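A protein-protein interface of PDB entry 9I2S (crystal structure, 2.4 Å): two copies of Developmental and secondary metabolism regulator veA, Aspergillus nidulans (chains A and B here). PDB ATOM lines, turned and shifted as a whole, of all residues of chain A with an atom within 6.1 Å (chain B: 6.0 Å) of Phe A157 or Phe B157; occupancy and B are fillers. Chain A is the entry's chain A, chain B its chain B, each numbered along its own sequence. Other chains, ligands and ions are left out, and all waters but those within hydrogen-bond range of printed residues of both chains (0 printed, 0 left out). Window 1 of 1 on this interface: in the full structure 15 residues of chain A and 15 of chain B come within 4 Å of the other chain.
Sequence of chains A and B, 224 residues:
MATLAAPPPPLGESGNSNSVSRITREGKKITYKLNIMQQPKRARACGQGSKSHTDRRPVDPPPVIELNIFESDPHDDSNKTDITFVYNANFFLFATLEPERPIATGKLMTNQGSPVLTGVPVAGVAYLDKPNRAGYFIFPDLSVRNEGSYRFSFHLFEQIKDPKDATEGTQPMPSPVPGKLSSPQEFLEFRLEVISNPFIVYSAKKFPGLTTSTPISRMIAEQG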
ATOM      1  N   ASN A  90     -39.297 -11.914 -21.257  1.00  0.00           N
ATOM      2  CA  ASN A  90     -38.394 -11.875 -22.402  1.00  0.00           C
ATOM      3  C   ASN A  90     -37.614 -13.177 -22.473  1.00  0.00           C
ATOM      4  O   ASN A  90     -37.264 -13.758 -21.441  1.00  0.00           O
ATOM      5  CB  ASN A  90     -37.427 -10.696 -22.316  1.00  0.00           C
ATOM      6  CG  ASN A  90     -38.136  -9.365 -22.327  1.00  0.00           C
ATOM      7  OD1 ASN A  90     -38.036  -8.593 -21.374  1.00  0.00           O
ATOM      8  ND2 ASN A  90     -38.888  -9.100 -23.391  1.00  0.00           N
ATOM      9  N   PHE A  91     -37.348 -13.640 -23.691  1.00  0.00           N
ATOM     10  CA  PHE A  91     -36.618 -14.882 -23.894  1.00  0.00           C
ATOM     11  C   PHE A  91     -35.529 -14.677 -24.936  1.00  0.00           C
ATOM     12  O   PHE A  91     -35.758 -14.034 -25.965  1.00  0.00           O
ATOM     13  CB  PHE A  91     -37.547 -16.011 -24.337  1.00  0.00           C
ATOM     14  CG  PHE A  91     -38.376 -16.588 -23.227  1.00  0.00           C
ATOM     15  CD1 PHE A  91     -37.825 -17.474 -22.317  1.00  0.00           C
ATOM     16  CD2 PHE A  91     -39.717 -16.262 -23.112  1.00  0.00           C
ATOM     17  CE1 PHE A  91     -38.592 -18.011 -21.302  1.00  0.00           C
ATOM     18  CE2 PHE A  91     -40.490 -16.796 -22.103  1.00  0.00           C
ATOM     19  CZ  PHE A  91     -39.925 -17.672 -21.194  1.00  0.00           C
ATOM     20  N   PHE A  92     -34.343 -15.217 -24.667  1.00  0.00           N
ATOM     21  CA  PHE A  92     -33.250 -15.184 -25.623  1.00  0.00           C
ATOM     22  C   PHE A  92     -32.652 -16.578 -25.705  1.00  0.00           C
ATOM     23  O   PHE A  92     -32.633 -17.317 -24.717  1.00  0.00           O
ATOM     24  CB  PHE A  92     -32.172 -14.158 -25.223  1.00  0.00           C
ATOM     25  CG  PHE A  92     -32.725 -12.792 -24.918  1.00  0.00           C
ATOM     26  CD1 PHE A  92     -33.147 -12.472 -23.638  1.00  0.00           C
ATOM     27  CD2 PHE A  92     -32.833 -11.836 -25.912  1.00  0.00           C
ATOM     28  CE1 PHE A  92     -33.665 -11.222 -23.356  1.00  0.00           C
ATOM     29  CE2 PHE A  92     -33.352 -10.582 -25.636  1.00  0.00           C
ATOM     30  CZ  PHE A  92     -33.768 -10.277 -24.359  1.00  0.00           C
ATOM     31  N   LEU A  93     -32.144 -16.925 -26.882  1.00  0.00           N
ATOM     32  CA  LEU A  93     -31.486 -18.204 -27.105  1.00  0.00           C
ATOM     33  C   LEU A  93     -30.094 -17.961 -27.658  1.00  0.00           C
ATOM     34  O   LEU A  93     -29.932 -17.274 -28.671  1.00  0.00           O
ATOM     35  CB  LEU A  93     -32.299 -19.088 -28.054  1.00  0.00           C
ATOM     36  CG  LEU A  93     -32.007 -20.579 -27.935  1.00  0.00           C
ATOM     37  CD1 LEU A  93     -32.461 -21.127 -26.586  1.00  0.00           C
ATOM     38  CD2 LEU A  93     -32.662 -21.328 -29.087  1.00  0.00           C
ATOM     39  N   PHE A  94     -29.102 -18.541 -26.993  1.00  0.00           N
ATOM     40  CA  PHE A  94     -27.696 -18.326 -27.286  1.00  0.00           C
ATOM     41  C   PHE A  94     -27.072 -19.623 -27.778  1.00  0.00           C
ATOM     42  O   PHE A  94     -27.267 -20.684 -27.175  1.00  0.00           O
ATOM     43  CB  PHE A  94     -26.973 -17.813 -26.033  1.00  0.00           C
ATOM     44  CG  PHE A  94     -25.486 -17.673 -26.188  1.00  0.00           C
ATOM     45  CD1 PHE A  94     -24.947 -16.900 -27.204  1.00  0.00           C
ATOM     46  CD2 PHE A  94     -24.625 -18.296 -25.298  1.00  0.00           C
ATOM     47  CE1 PHE A  94     -23.576 -16.759 -27.338  1.00  0.00           C
ATOM     48  CE2 PHE A  94     -23.252 -18.153 -25.422  1.00  0.00           C
ATOM     49  CZ  PHE A  94     -22.729 -17.387 -26.445  1.00  0.00           C
ATOM     50  N   VAL A 122     -27.076 -14.924 -30.867  1.00  0.00           N
ATOM     51  CA  VAL A 122     -28.201 -14.689 -29.967  1.00  0.00           C
ATOM     52  C   VAL A 122     -29.450 -14.413 -30.796  1.00  0.00           C
ATOM     53  O   VAL A 122     -29.444 -13.531 -31.663  1.00  0.00           O
ATOM     54  CB  VAL A 122     -27.931 -13.525 -28.998  1.00  0.00           C
ATOM     55  CG1 VAL A 122     -29.160 -13.272 -28.152  1.00  0.00           C
ATOM     56  CG2 VAL A 122     -26.712 -13.816 -28.132  1.00  0.00           C
ATOM     57  N   HIS A 155     -28.689 -22.306 -25.403  1.00  0.00           N
ATOM     58  CA  HIS A 155     -28.962 -21.993 -24.008  1.00  0.00           C
ATOM     59  C   HIS A 155     -30.068 -20.954 -23.937  1.00  0.00           C
ATOM     60  O   HIS A 155     -29.965 -19.891 -24.557  1.00  0.00           O
ATOM     61  CB  HIS A 155     -27.690 -21.491 -23.315  1.00  0.00           C
ATOM     62  CG  HIS A 155     -26.452 -22.229 -23.724  1.00  0.00           C
ATOM     63  ND1 HIS A 155     -26.023 -23.375 -23.087  1.00  0.00           N
ATOM     64  CD2 HIS A 155     -25.578 -22.013 -24.735  1.00  0.00           C
ATOM     65  CE1 HIS A 155     -24.923 -23.817 -23.671  1.00  0.00           C
ATOM     66  NE2 HIS A 155     -24.633 -23.010 -24.675  1.00  0.00           N
ATOM     67  N   LEU A 156     -31.096 -21.235 -23.142  1.00  0.00           N
ATOM     68  CA  LEU A 156     -32.237 -20.343 -23.022  1.00  0.00           C
ATOM     69  C   LEU A 156     -32.071 -19.437 -21.815  1.00  0.00           C
ATOM     70  O   LEU A 156     -31.797 -19.908 -20.708  1.00  0.00           O
ATOM     71  CB  LEU A 156     -33.536 -21.141 -22.901  1.00  0.00           C
ATOM     72  CG  LEU A 156     -34.785 -20.272 -22.753  1.00  0.00           C
ATOM     73  CD1 LEU A 156     -35.014 -19.482 -24.029  1.00  0.00           C
ATOM     74  CD2 LEU A 156     -36.003 -21.110 -22.407  1.00  0.00           C
ATOM     75  N   PHE A 157     -32.256 -18.140 -22.030  1.00  0.00           N
ATOM     76  CA  PHE A 157     -32.233 -17.145 -20.969  1.00  0.00           C
ATOM     77  C   PHE A 157     -33.602 -16.496 -20.845  1.00  0.00           C
ATOM     78  O   PHE A 157     -34.202 -16.101 -21.852  1.00  0.00           O
ATOM     79  CB  PHE A 157     -31.167 -16.090 -21.236  1.00  0.00           C
ATOM     80  CG  PHE A 157     -29.777 -16.630 -21.233  1.00  0.00           C
ATOM     81  CD1 PHE A 157     -29.197 -17.080 -20.057  1.00  0.00           C
ATOM     82  CD2 PHE A 157     -29.057 -16.710 -22.408  1.00  0.00           C
ATOM     83  CE1 PHE A 157     -27.913 -17.578 -20.057  1.00  0.00           C
ATOM     84  CE2 PHE A 157     -27.779 -17.207 -22.416  1.00  0.00           C
ATOM     85  CZ  PHE A 157     -27.203 -17.644 -21.242  1.00  0.00           C
ATOM     86  N   GLU A 158     -34.087 -16.383 -19.617  1.00  0.00           N
ATOM     87  CA  GLU A 158     -35.368 -15.760 -19.333  1.00  0.00           C
ATOM     88  C   GLU A 158     -35.175 -14.468 -18.552  1.00  0.00           C
ATOM     89  O   GLU A 158     -34.359 -14.403 -17.628  1.00  0.00           O
ATOM     90  CB  GLU A 158     -36.285 -16.705 -18.549  1.00  0.00           C
ATOM     91  CG  GLU A 158     -37.623 -16.082 -18.166  1.00  0.00           C
ATOM     92  CD  GLU A 158     -38.517 -17.042 -17.406  1.00  0.00           C
ATOM     93  OE1 GLU A 158     -38.139 -18.223 -17.280  1.00  0.00           O
ATOM     94  OE2 GLU A 158     -39.591 -16.620 -16.932  1.00  0.00           O
ATOM     95  N   GLN A 159     -35.914 -13.438 -18.946  1.00  0.00           N
ATOM     96  CA  GLN A 159     -35.897 -12.135 -18.293  1.00  0.00           C
ATOM     97  C   GLN A 159     -37.314 -11.856 -17.808  1.00  0.00           C
ATOM     98  O   GLN A 159     -38.209 -11.579 -18.614  1.00  0.00           O
ATOM     99  CB  GLN A 159     -35.409 -11.045 -19.242  1.00  0.00           C
ATOM    100  CG  GLN A 159     -34.296 -10.177 -18.695  1.00  0.00           C
ATOM    101  CD  GLN A 159     -33.962  -9.027 -19.616  1.00  0.00           C
ATOM    102  OE1 GLN A 159     -34.386  -9.007 -20.781  1.00  0.00           O
ATOM    103  NE2 GLN A 159     -33.259  -8.020 -19.079  1.00  0.00           N
ATOM    104  N   LEU A 188     -31.194 -11.669 -15.544  1.00  0.00           N
ATOM    105  CA  LEU A 188     -31.212 -12.671 -16.597  1.00  0.00           C
ATOM    106  C   LEU A 188     -31.014 -14.039 -15.964  1.00  0.00           C
ATOM    107  O   LEU A 188     -30.045 -14.245 -15.226  1.00  0.00           O
ATOM    108  CB  LEU A 188     -30.114 -12.395 -17.626  1.00  0.00           C
ATOM    109  CG  LEU A 188     -30.233 -13.034 -19.006  1.00  0.00           C
ATOM    110  CD1 LEU A 188     -31.320 -12.358 -19.843  1.00  0.00           C
ATOM    111  CD2 LEU A 188     -28.880 -12.986 -19.704  1.00  0.00           C
ATOM    112  N   GLU A 189     -31.914 -14.975 -16.261  1.00  0.00           N
ATOM    113  CA  GLU A 189     -31.872 -16.306 -15.664  1.00  0.00           C
ATOM    114  C   GLU A 189     -31.714 -17.362 -16.743  1.00  0.00           C
ATOM    115  O   GLU A 189     -32.519 -17.428 -17.678  1.00  0.00           O
ATOM    116  CB  GLU A 189     -33.128 -16.596 -14.841  1.00  0.00           C
ATOM    117  CG  GLU A 189     -33.162 -15.918 -13.491  1.00  0.00           C
ATOM    118  CD  GLU A 189     -34.076 -16.638 -12.518  1.00  0.00           C
ATOM    119  OE1 GLU A 189     -35.310 -16.591 -12.704  1.00  0.00           O
ATOM    120  OE2 GLU A 189     -33.556 -17.266 -11.572  1.00  0.00           O
ATOM    121  N   PHE A 190     -30.683 -18.190 -16.604  1.00  0.00           N
ATOM    122  CA  PHE A 190     -30.565 -19.374 -17.436  1.00  0.00           C
ATOM    123  C   PHE A 190     -31.648 -20.368 -17.043  1.00  0.00           C
ATOM    124  O   PHE A 190     -31.916 -20.578 -15.857  1.00  0.00           O
ATOM    125  CB  PHE A 190     -29.177 -19.995 -17.302  1.00  0.00           C
ATOM    126  CG  PHE A 190     -29.033 -21.304 -18.016  1.00  0.00           C
ATOM    127  CD1 PHE A 190     -28.828 -21.344 -19.386  1.00  0.00           C
ATOM    128  CD2 PHE A 190     -29.089 -22.501 -17.313  1.00  0.00           C
ATOM    129  CE1 PHE A 190     -28.703 -22.559 -20.052  1.00  0.00           C
ATOM    130  CE2 PHE A 190     -28.958 -23.716 -17.967  1.00  0.00           C
ATOM    131  CZ  PHE A 190     -28.764 -23.745 -19.339  1.00  0.00           C
ATOM    132  N   ARG A 191     -32.283 -20.973 -18.048  1.00  0.00           N
ATOM    133  CA  ARG A 191     -33.359 -21.925 -17.812  1.00  0.00           C
ATOM    134  C   ARG A 191     -32.968 -23.352 -18.169  1.00  0.00           C
ATOM    135  O   ARG A 191     -33.016 -24.232 -17.305  1.00  0.00           O
ATOM    136  CB  ARG A 191     -34.606 -21.501 -18.607  1.00  0.00           C
ATOM    137  CG  ARG A 191     -35.319 -20.297 -18.022  1.00  0.00           C
ATOM    138  CD  ARG A 191     -35.961 -20.655 -16.695  1.00  0.00           C
ATOM    139  NE  ARG A 191     -36.453 -19.483 -15.983  1.00  0.00           N
ATOM    140  CZ  ARG A 191     -36.072 -19.129 -14.763  1.00  0.00           C
ATOM    141  NH1 ARG A 191     -35.189 -19.842 -14.079  1.00  0.00           N
ATOM    142  NH2 ARG A 191     -36.599 -18.040 -14.210  1.00  0.00           N
ATOM    143  N   LEU A 192     -32.561 -23.610 -19.409  1.00  0.00           N
ATOM    144  CA  LEU A 192     -32.204 -24.966 -19.807  1.00  0.00           C
ATOM    145  C   LEU A 192     -31.412 -24.902 -21.104  1.00  0.00           C
ATOM    146  O   LEU A 192     -31.221 -23.835 -21.693  1.00  0.00           O
ATOM    147  CB  LEU A 192     -33.447 -25.846 -19.979  1.00  0.00           C
ATOM    148  CG  LEU A 192     -34.256 -25.687 -21.274  1.00  0.00           C
ATOM    149  CD1 LEU A 192     -34.906 -27.018 -21.634  1.00  0.00           C
ATOM    150  CD2 LEU A 192     -35.279 -24.573 -21.188  1.00  0.00           C
ATOM    151  N   ASN B  90     -26.422  -2.672 -19.492  1.00  0.00           N
ATOM    152  CA  ASN B  90     -26.380  -3.810 -18.586  1.00  0.00           C
ATOM    153  C   ASN B  90     -25.451  -4.877 -19.142  1.00  0.00           C
ATOM    154  O   ASN B  90     -25.303  -5.031 -20.358  1.00  0.00           O
ATOM    155  CB  ASN B  90     -27.776  -4.400 -18.365  1.00  0.00           C
ATOM    156  CG  ASN B  90     -28.724  -3.428 -17.695  1.00  0.00           C
ATOM    157  OD1 ASN B  90     -28.300  -2.427 -17.120  1.00  0.00           O
ATOM    158  ND2 ASN B  90     -30.020  -3.714 -17.773  1.00  0.00           N
ATOM    159  N   PHE B  91     -24.815  -5.615 -18.241  1.00  0.00           N
ATOM    160  CA  PHE B  91     -23.887  -6.661 -18.632  1.00  0.00           C
ATOM    161  C   PHE B  91     -24.201  -7.927 -17.858  1.00  0.00           C
ATOM    162  O   PHE B  91     -24.574  -7.872 -16.683  1.00  0.00           O
ATOM    163  CB  PHE B  91     -22.428  -6.256 -18.388  1.00  0.00           C
ATOM    164  CG  PHE B  91     -21.880  -5.313 -19.420  1.00  0.00           C
ATOM    165  CD1 PHE B  91     -21.584  -5.756 -20.698  1.00  0.00           C
ATOM    166  CD2 PHE B  91     -21.639  -3.985 -19.104  1.00  0.00           C
ATOM    167  CE1 PHE B  91     -21.077  -4.889 -21.650  1.00  0.00           C
ATOM    168  CE2 PHE B  91     -21.127  -3.115 -20.048  1.00  0.00           C
ATOM    169  CZ  PHE B  91     -20.846  -3.568 -21.322  1.00  0.00           C
ATOM    170  N   PHE B  92     -24.076  -9.062 -18.528  1.00  0.00           N
ATOM    171  CA  PHE B  92     -24.229 -10.352 -17.883  1.00  0.00           C
ATOM    172  C   PHE B  92     -23.081 -11.241 -18.335  1.00  0.00           C
ATOM    173  O   PHE B  92     -22.601 -11.132 -19.466  1.00  0.00           O
ATOM    174  CB  PHE B  92     -25.589 -10.985 -18.209  1.00  0.00           C
ATOM    175  CG  PHE B  92     -26.763 -10.106 -17.866  1.00  0.00           C
ATOM    176  CD1 PHE B  92     -27.293 -10.096 -16.584  1.00  0.00           C
ATOM    177  CD2 PHE B  92     -27.337  -9.291 -18.827  1.00  0.00           C
ATOM    178  CE1 PHE B  92     -28.372  -9.284 -16.268  1.00  0.00           C
ATOM    179  CE2 PHE B  92     -28.418  -8.481 -18.519  1.00  0.00           C
ATOM    180  CZ  PHE B  92     -28.935  -8.476 -17.238  1.00  0.00           C
ATOM    181  N   LEU B  93     -22.655 -12.141 -17.459  1.00  0.00           N
ATOM    182  CA  LEU B  93     -21.614 -13.097 -17.794  1.00  0.00           C
ATOM    183  C   LEU B  93     -22.149 -14.495 -17.556  1.00  0.00           C
ATOM    184  O   LEU B  93     -22.623 -14.808 -16.457  1.00  0.00           O
ATOM    185  CB  LEU B  93     -20.340 -12.846 -16.978  1.00  0.00           C
ATOM    186  CG  LEU B  93     -19.054 -13.408 -17.589  1.00  0.00           C
ATOM    187  CD1 LEU B  93     -18.734 -12.729 -18.916  1.00  0.00           C
ATOM    188  CD2 LEU B  93     -17.899 -13.244 -16.623  1.00  0.00           C
ATOM    189  N   PHE B  94     -22.050 -15.335 -18.579  1.00  0.00           N
ATOM    190  CA  PHE B  94     -22.633 -16.666 -18.572  1.00  0.00           C
ATOM    191  C   PHE B  94     -21.528 -17.705 -18.593  1.00  0.00           C
ATOM    192  O   PHE B  94     -20.619 -17.633 -19.428  1.00  0.00           O
ATOM    193  CB  PHE B  94     -23.570 -16.837 -19.774  1.00  0.00           C
ATOM    194  CG  PHE B  94     -24.197 -18.198 -19.879  1.00  0.00           C
ATOM    195  CD1 PHE B  94     -24.912 -18.735 -18.822  1.00  0.00           C
ATOM    196  CD2 PHE B  94     -24.111 -18.921 -21.063  1.00  0.00           C
ATOM    197  CE1 PHE B  94     -25.503 -19.979 -18.926  1.00  0.00           C
ATOM    198  CE2 PHE B  94     -24.714 -20.163 -21.183  1.00  0.00           C
ATOM    199  CZ  PHE B  94     -25.407 -20.695 -20.111  1.00  0.00           C
ATOM    200  N   VAL B 122     -25.217 -17.452 -14.349  1.00  0.00           N
ATOM    201  CA  VAL B 122     -25.281 -16.080 -14.842  1.00  0.00           C
ATOM    202  C   VAL B 122     -24.899 -15.147 -13.703  1.00  0.00           C
ATOM    203  O   VAL B 122     -25.489 -15.204 -12.617  1.00  0.00           O
ATOM    204  CB  VAL B 122     -26.668 -15.726 -15.404  1.00  0.00           C
ATOM    205  CG1 VAL B 122     -26.724 -14.245 -15.761  1.00  0.00           C
ATOM    206  CG2 VAL B 122     -26.949 -16.564 -16.628  1.00  0.00           C
ATOM    207  N   HIS B 155     -19.037 -16.147 -21.202  1.00  0.00           N
ATOM    208  CA  HIS B 155     -19.541 -15.396 -22.347  1.00  0.00           C
ATOM    209  C   HIS B 155     -20.206 -14.115 -21.862  1.00  0.00           C
ATOM    210  O   HIS B 155     -21.043 -14.154 -20.957  1.00  0.00           O
ATOM    211  CB  HIS B 155     -20.546 -16.236 -23.142  1.00  0.00           C
ATOM    212  CG  HIS B 155     -20.184 -17.686 -23.248  1.00  0.00           C
ATOM    213  ND1 HIS B 155     -19.381 -18.182 -24.255  1.00  0.00           N
ATOM    214  CD2 HIS B 155     -20.462 -18.738 -22.440  1.00  0.00           C
ATOM    215  CE1 HIS B 155     -19.220 -19.483 -24.087  1.00  0.00           C
ATOM    216  NE2 HIS B 155     -19.858 -19.843 -22.989  1.00  0.00           N
ATOM    217  N   LEU B 156     -19.846 -12.987 -22.474  1.00  0.00           N
ATOM    218  CA  LEU B 156     -20.347 -11.681 -22.063  1.00  0.00           C
ATOM    219  C   LEU B 156     -21.516 -11.262 -22.948  1.00  0.00           C
ATOM    220  O   LEU B 156     -21.417 -11.309 -24.180  1.00  0.00           O
ATOM    221  CB  LEU B 156     -19.234 -10.636 -22.139  1.00  0.00           C
ATOM    222  CG  LEU B 156     -19.642  -9.221 -21.737  1.00  0.00           C
ATOM    223  CD1 LEU B 156     -20.044  -9.181 -20.269  1.00  0.00           C
ATOM    224  CD2 LEU B 156     -18.514  -8.235 -22.030  1.00  0.00           C
ATOM    225  N   PHE B 157     -22.615 -10.859 -22.315  1.00  0.00           N
ATOM    226  CA  PHE B 157     -23.800 -10.346 -22.989  1.00  0.00           C
ATOM    227  C   PHE B 157     -23.997  -8.888 -22.598  1.00  0.00           C
ATOM    228  O   PHE B 157     -23.896  -8.545 -21.411  1.00  0.00           O
ATOM    229  CB  PHE B 157     -25.032 -11.175 -22.614  1.00  0.00           C
ATOM    230  CG  PHE B 157     -24.949 -12.597 -23.078  1.00  0.00           C
ATOM    231  CD1 PHE B 157     -24.876 -12.887 -24.427  1.00  0.00           C
ATOM    232  CD2 PHE B 157     -24.926 -13.645 -22.170  1.00  0.00           C
ATOM    233  CE1 PHE B 157     -24.777 -14.189 -24.867  1.00  0.00           C
ATOM    234  CE2 PHE B 157     -24.833 -14.958 -22.607  1.00  0.00           C
ATOM    235  CZ  PHE B 157     -24.756 -15.226 -23.957  1.00  0.00           C
ATOM    236  N   GLU B 158     -24.254  -8.039 -23.585  1.00  0.00           N
ATOM    237  CA  GLU B 158     -24.481  -6.619 -23.381  1.00  0.00           C
ATOM    238  C   GLU B 158     -25.935  -6.317 -23.717  1.00  0.00           C
ATOM    239  O   GLU B 158     -26.381  -6.597 -24.834  1.00  0.00           O
ATOM    240  CB  GLU B 158     -23.537  -5.785 -24.249  1.00  0.00           C
ATOM    241  CG  GLU B 158     -23.818  -4.320 -24.200  1.00  0.00           C
ATOM    242  CD  GLU B 158     -22.842  -3.522 -25.026  1.00  0.00           C
ATOM    243  OE1 GLU B 158     -21.790  -4.064 -25.437  1.00  0.00           O
ATOM    244  OE2 GLU B 158     -23.167  -2.354 -25.299  1.00  0.00           O
ATOM    245  N   GLN B 159     -26.673  -5.768 -22.752  1.00  0.00           N
ATOM    246  CA  GLN B 159     -28.056  -5.349 -22.952  1.00  0.00           C
ATOM    247  C   GLN B 159     -28.004  -3.833 -23.088  1.00  0.00           C
ATOM    248  O   GLN B 159     -27.699  -3.143 -22.114  1.00  0.00           O
ATOM    249  CB  GLN B 159     -28.948  -5.733 -21.774  1.00  0.00           C
ATOM    250  CG  GLN B 159     -30.203  -4.887 -21.655  1.00  0.00           C
ATOM    251  CD  GLN B 159     -31.243  -5.596 -20.865  1.00  0.00           C
ATOM    252  OE1 GLN B 159     -30.889  -6.371 -19.952  1.00  0.00           O
ATOM    253  NE2 GLN B 159     -32.520  -5.432 -21.259  1.00  0.00           N
ATOM    254  N   LEU B 188     -30.392  -8.766 -26.576  1.00  0.00           N
ATOM    255  CA  LEU B 188     -29.144  -9.194 -25.973  1.00  0.00           C
ATOM    256  C   LEU B 188     -28.105  -9.402 -27.064  1.00  0.00           C
ATOM    257  O   LEU B 188     -28.370 -10.095 -28.052  1.00  0.00           O
ATOM    258  CB  LEU B 188     -29.351 -10.497 -25.199  1.00  0.00           C
ATOM    259  CG  LEU B 188     -29.202 -10.483 -23.681  1.00  0.00           C
ATOM    260  CD1 LEU B 188     -28.960 -11.895 -23.181  1.00  0.00           C
ATOM    261  CD2 LEU B 188     -28.095  -9.536 -23.241  1.00  0.00           C
ATOM    262  N   GLU B 189     -26.928  -8.810 -26.887  1.00  0.00           N
ATOM    263  CA  GLU B 189     -25.834  -8.934 -27.842  1.00  0.00           C
ATOM    264  C   GLU B 189     -24.647  -9.622 -27.192  1.00  0.00           C
ATOM    265  O   GLU B 189     -24.180  -9.198 -26.131  1.00  0.00           O
ATOM    266  CB  GLU B 189     -25.405  -7.590 -28.434  1.00  0.00           C
ATOM    267  CG  GLU B 189     -26.532  -6.788 -29.045  1.00  0.00           C
ATOM    268  CD  GLU B 189     -26.054  -5.960 -30.222  1.00  0.00           C
ATOM    269  OE1 GLU B 189     -25.060  -6.365 -30.865  1.00  0.00           O
ATOM    270  OE2 GLU B 189     -26.672  -4.916 -30.515  1.00  0.00           O
ATOM    271  N   PHE B 190     -24.176 -10.688 -27.827  1.00  0.00           N
ATOM    272  CA  PHE B 190     -22.942 -11.331 -27.408  1.00  0.00           C
ATOM    273  C   PHE B 190     -21.749 -10.481 -27.827  1.00  0.00           C
ATOM    274  O   PHE B 190     -21.727  -9.908 -28.919  1.00  0.00           O
ATOM    275  CB  PHE B 190     -22.842 -12.720 -28.030  1.00  0.00           C
ATOM    276  CG  PHE B 190     -21.519 -13.389 -27.817  1.00  0.00           C
ATOM    277  CD1 PHE B 190     -21.181 -13.903 -26.573  1.00  0.00           C
ATOM    278  CD2 PHE B 190     -20.609 -13.500 -28.861  1.00  0.00           C
ATOM    279  CE1 PHE B 190     -19.962 -14.524 -26.374  1.00  0.00           C
ATOM    280  CE2 PHE B 190     -19.387 -14.120 -28.670  1.00  0.00           C
ATOM    281  CZ  PHE B 190     -19.063 -14.634 -27.423  1.00  0.00           C
ATOM    282  N   ARG B 191     -20.739 -10.414 -26.960  1.00  0.00           N
ATOM    283  CA  ARG B 191     -19.548  -9.627 -27.245  1.00  0.00           C
ATOM    284  C   ARG B 191     -18.308 -10.499 -27.384  1.00  0.00           C
ATOM    285  O   ARG B 191     -17.658 -10.486 -28.434  1.00  0.00           O
ATOM    286  CB  ARG B 191     -19.336  -8.582 -26.142  1.00  0.00           C
ATOM    287  CG  ARG B 191     -20.399  -7.504 -26.093  1.00  0.00           C
ATOM    288  CD  ARG B 191     -20.245  -6.541 -27.249  1.00  0.00           C
ATOM    289  NE  ARG B 191     -21.346  -5.591 -27.309  1.00  0.00           N
ATOM    290  CZ  ARG B 191     -22.070  -5.347 -28.392  1.00  0.00           C
ATOM    291  NH1 ARG B 191     -21.824  -5.956 -29.540  1.00  0.00           N
ATOM    292  NH2 ARG B 191     -23.060  -4.462 -28.322  1.00  0.00           N
ATOM    293  N   LEU B 192     -17.961 -11.268 -26.358  1.00  0.00           N
ATOM    294  CA  LEU B 192     -16.757 -12.085 -26.408  1.00  0.00           C
ATOM    295  C   LEU B 192     -16.785 -13.064 -25.247  1.00  0.00           C
ATOM    296  O   LEU B 192     -17.579 -12.932 -24.311  1.00  0.00           O
ATOM    297  CB  LEU B 192     -15.483 -11.229 -26.366  1.00  0.00           C
ATOM    298  CG  LEU B 192     -14.998 -10.756 -24.996  1.00  0.00           C
ATOM    299  CD1 LEU B 192     -13.564 -10.258 -25.071  1.00  0.00           C
ATOM    300  CD2 LEU B 192     -15.928  -9.665 -24.487  1.00  0.00           C
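Phe A157 touches just these residues of chain B: Phe B94, Val B122 and Phe B157. Of chain A, only Phe A94, Val A122 and Phe A157 come within 4 Å of Phe B157. Printed residues of chain B within 4 Å of Phe A190: Phe B94. Of the printed residues of chain A, Phe B94 touches His A155 (3.7 Å), Phe A157 (3.3 Å) and Phe A190 (3.6 Å). The nearest residue of chain B that does not touch Phe A157 is Leu B188 (4.9 Å).
Of the 16 printed residues of chain A, 8 touch a printed residue of chain B. Along chain A the printed residues that touch a printed residue of chain B span positions 92 to 190.
Among the printed residues, merely in contact across the chains: Val A122 with Leu B188, Phe A157 with Phe B94, Phe A94 with Phe B157, Leu A188 with Val B122, Phe A190 with Phe B94, Phe A92 with Leu B188, Leu A188 with Leu B188, Phe A157 with Val B122, His A155 with Phe B94, Phe A157 with Phe B157, Leu A188 with Phe B92, Phe A94 with His B155, Phe A94 with Phe B190 and Val A122 with Phe B157.
The backbone carbonyl oxygen (O) of Asn A90 is in hydrogen-bond range of the backbone NH (N) of Gln A159, 2.9 Å away. The backbone carbonyl oxygen (O) of Phe A92 lies within hydrogen-bond range of the backbone NH (N) of Phe A157 (2.8 Å). The backbone carbonyl oxygen (O) of Phe A94 is in hydrogen-bond range of the backbone NH (N) of His A155, at 2.8 Å. N of Gln B159 sits at hydrogen-bond distance from O of Asn B90 (2.9 Å). O of Phe B92 is in hydrogen-bond range of N of Phe B157, at 2.9 Å. The backbone carbonyl oxygen of Phe B94 lies within hydrogen-bond range of the backbone NH of His B155 (2.8 Å).
NE2 of Gln A159 is in hydrogen-bond range of OE1 of Gln B159, 3.0 Å away.
Val A122 touches Leu B188, and with the chains exchanged Leu A188 touches Val B122. Phe A157 touches its own counterpart, Phe B157. Gln A159 touches its own counterpart, Gln B159. Leu B188 touches its own counterpart, Leu A188.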
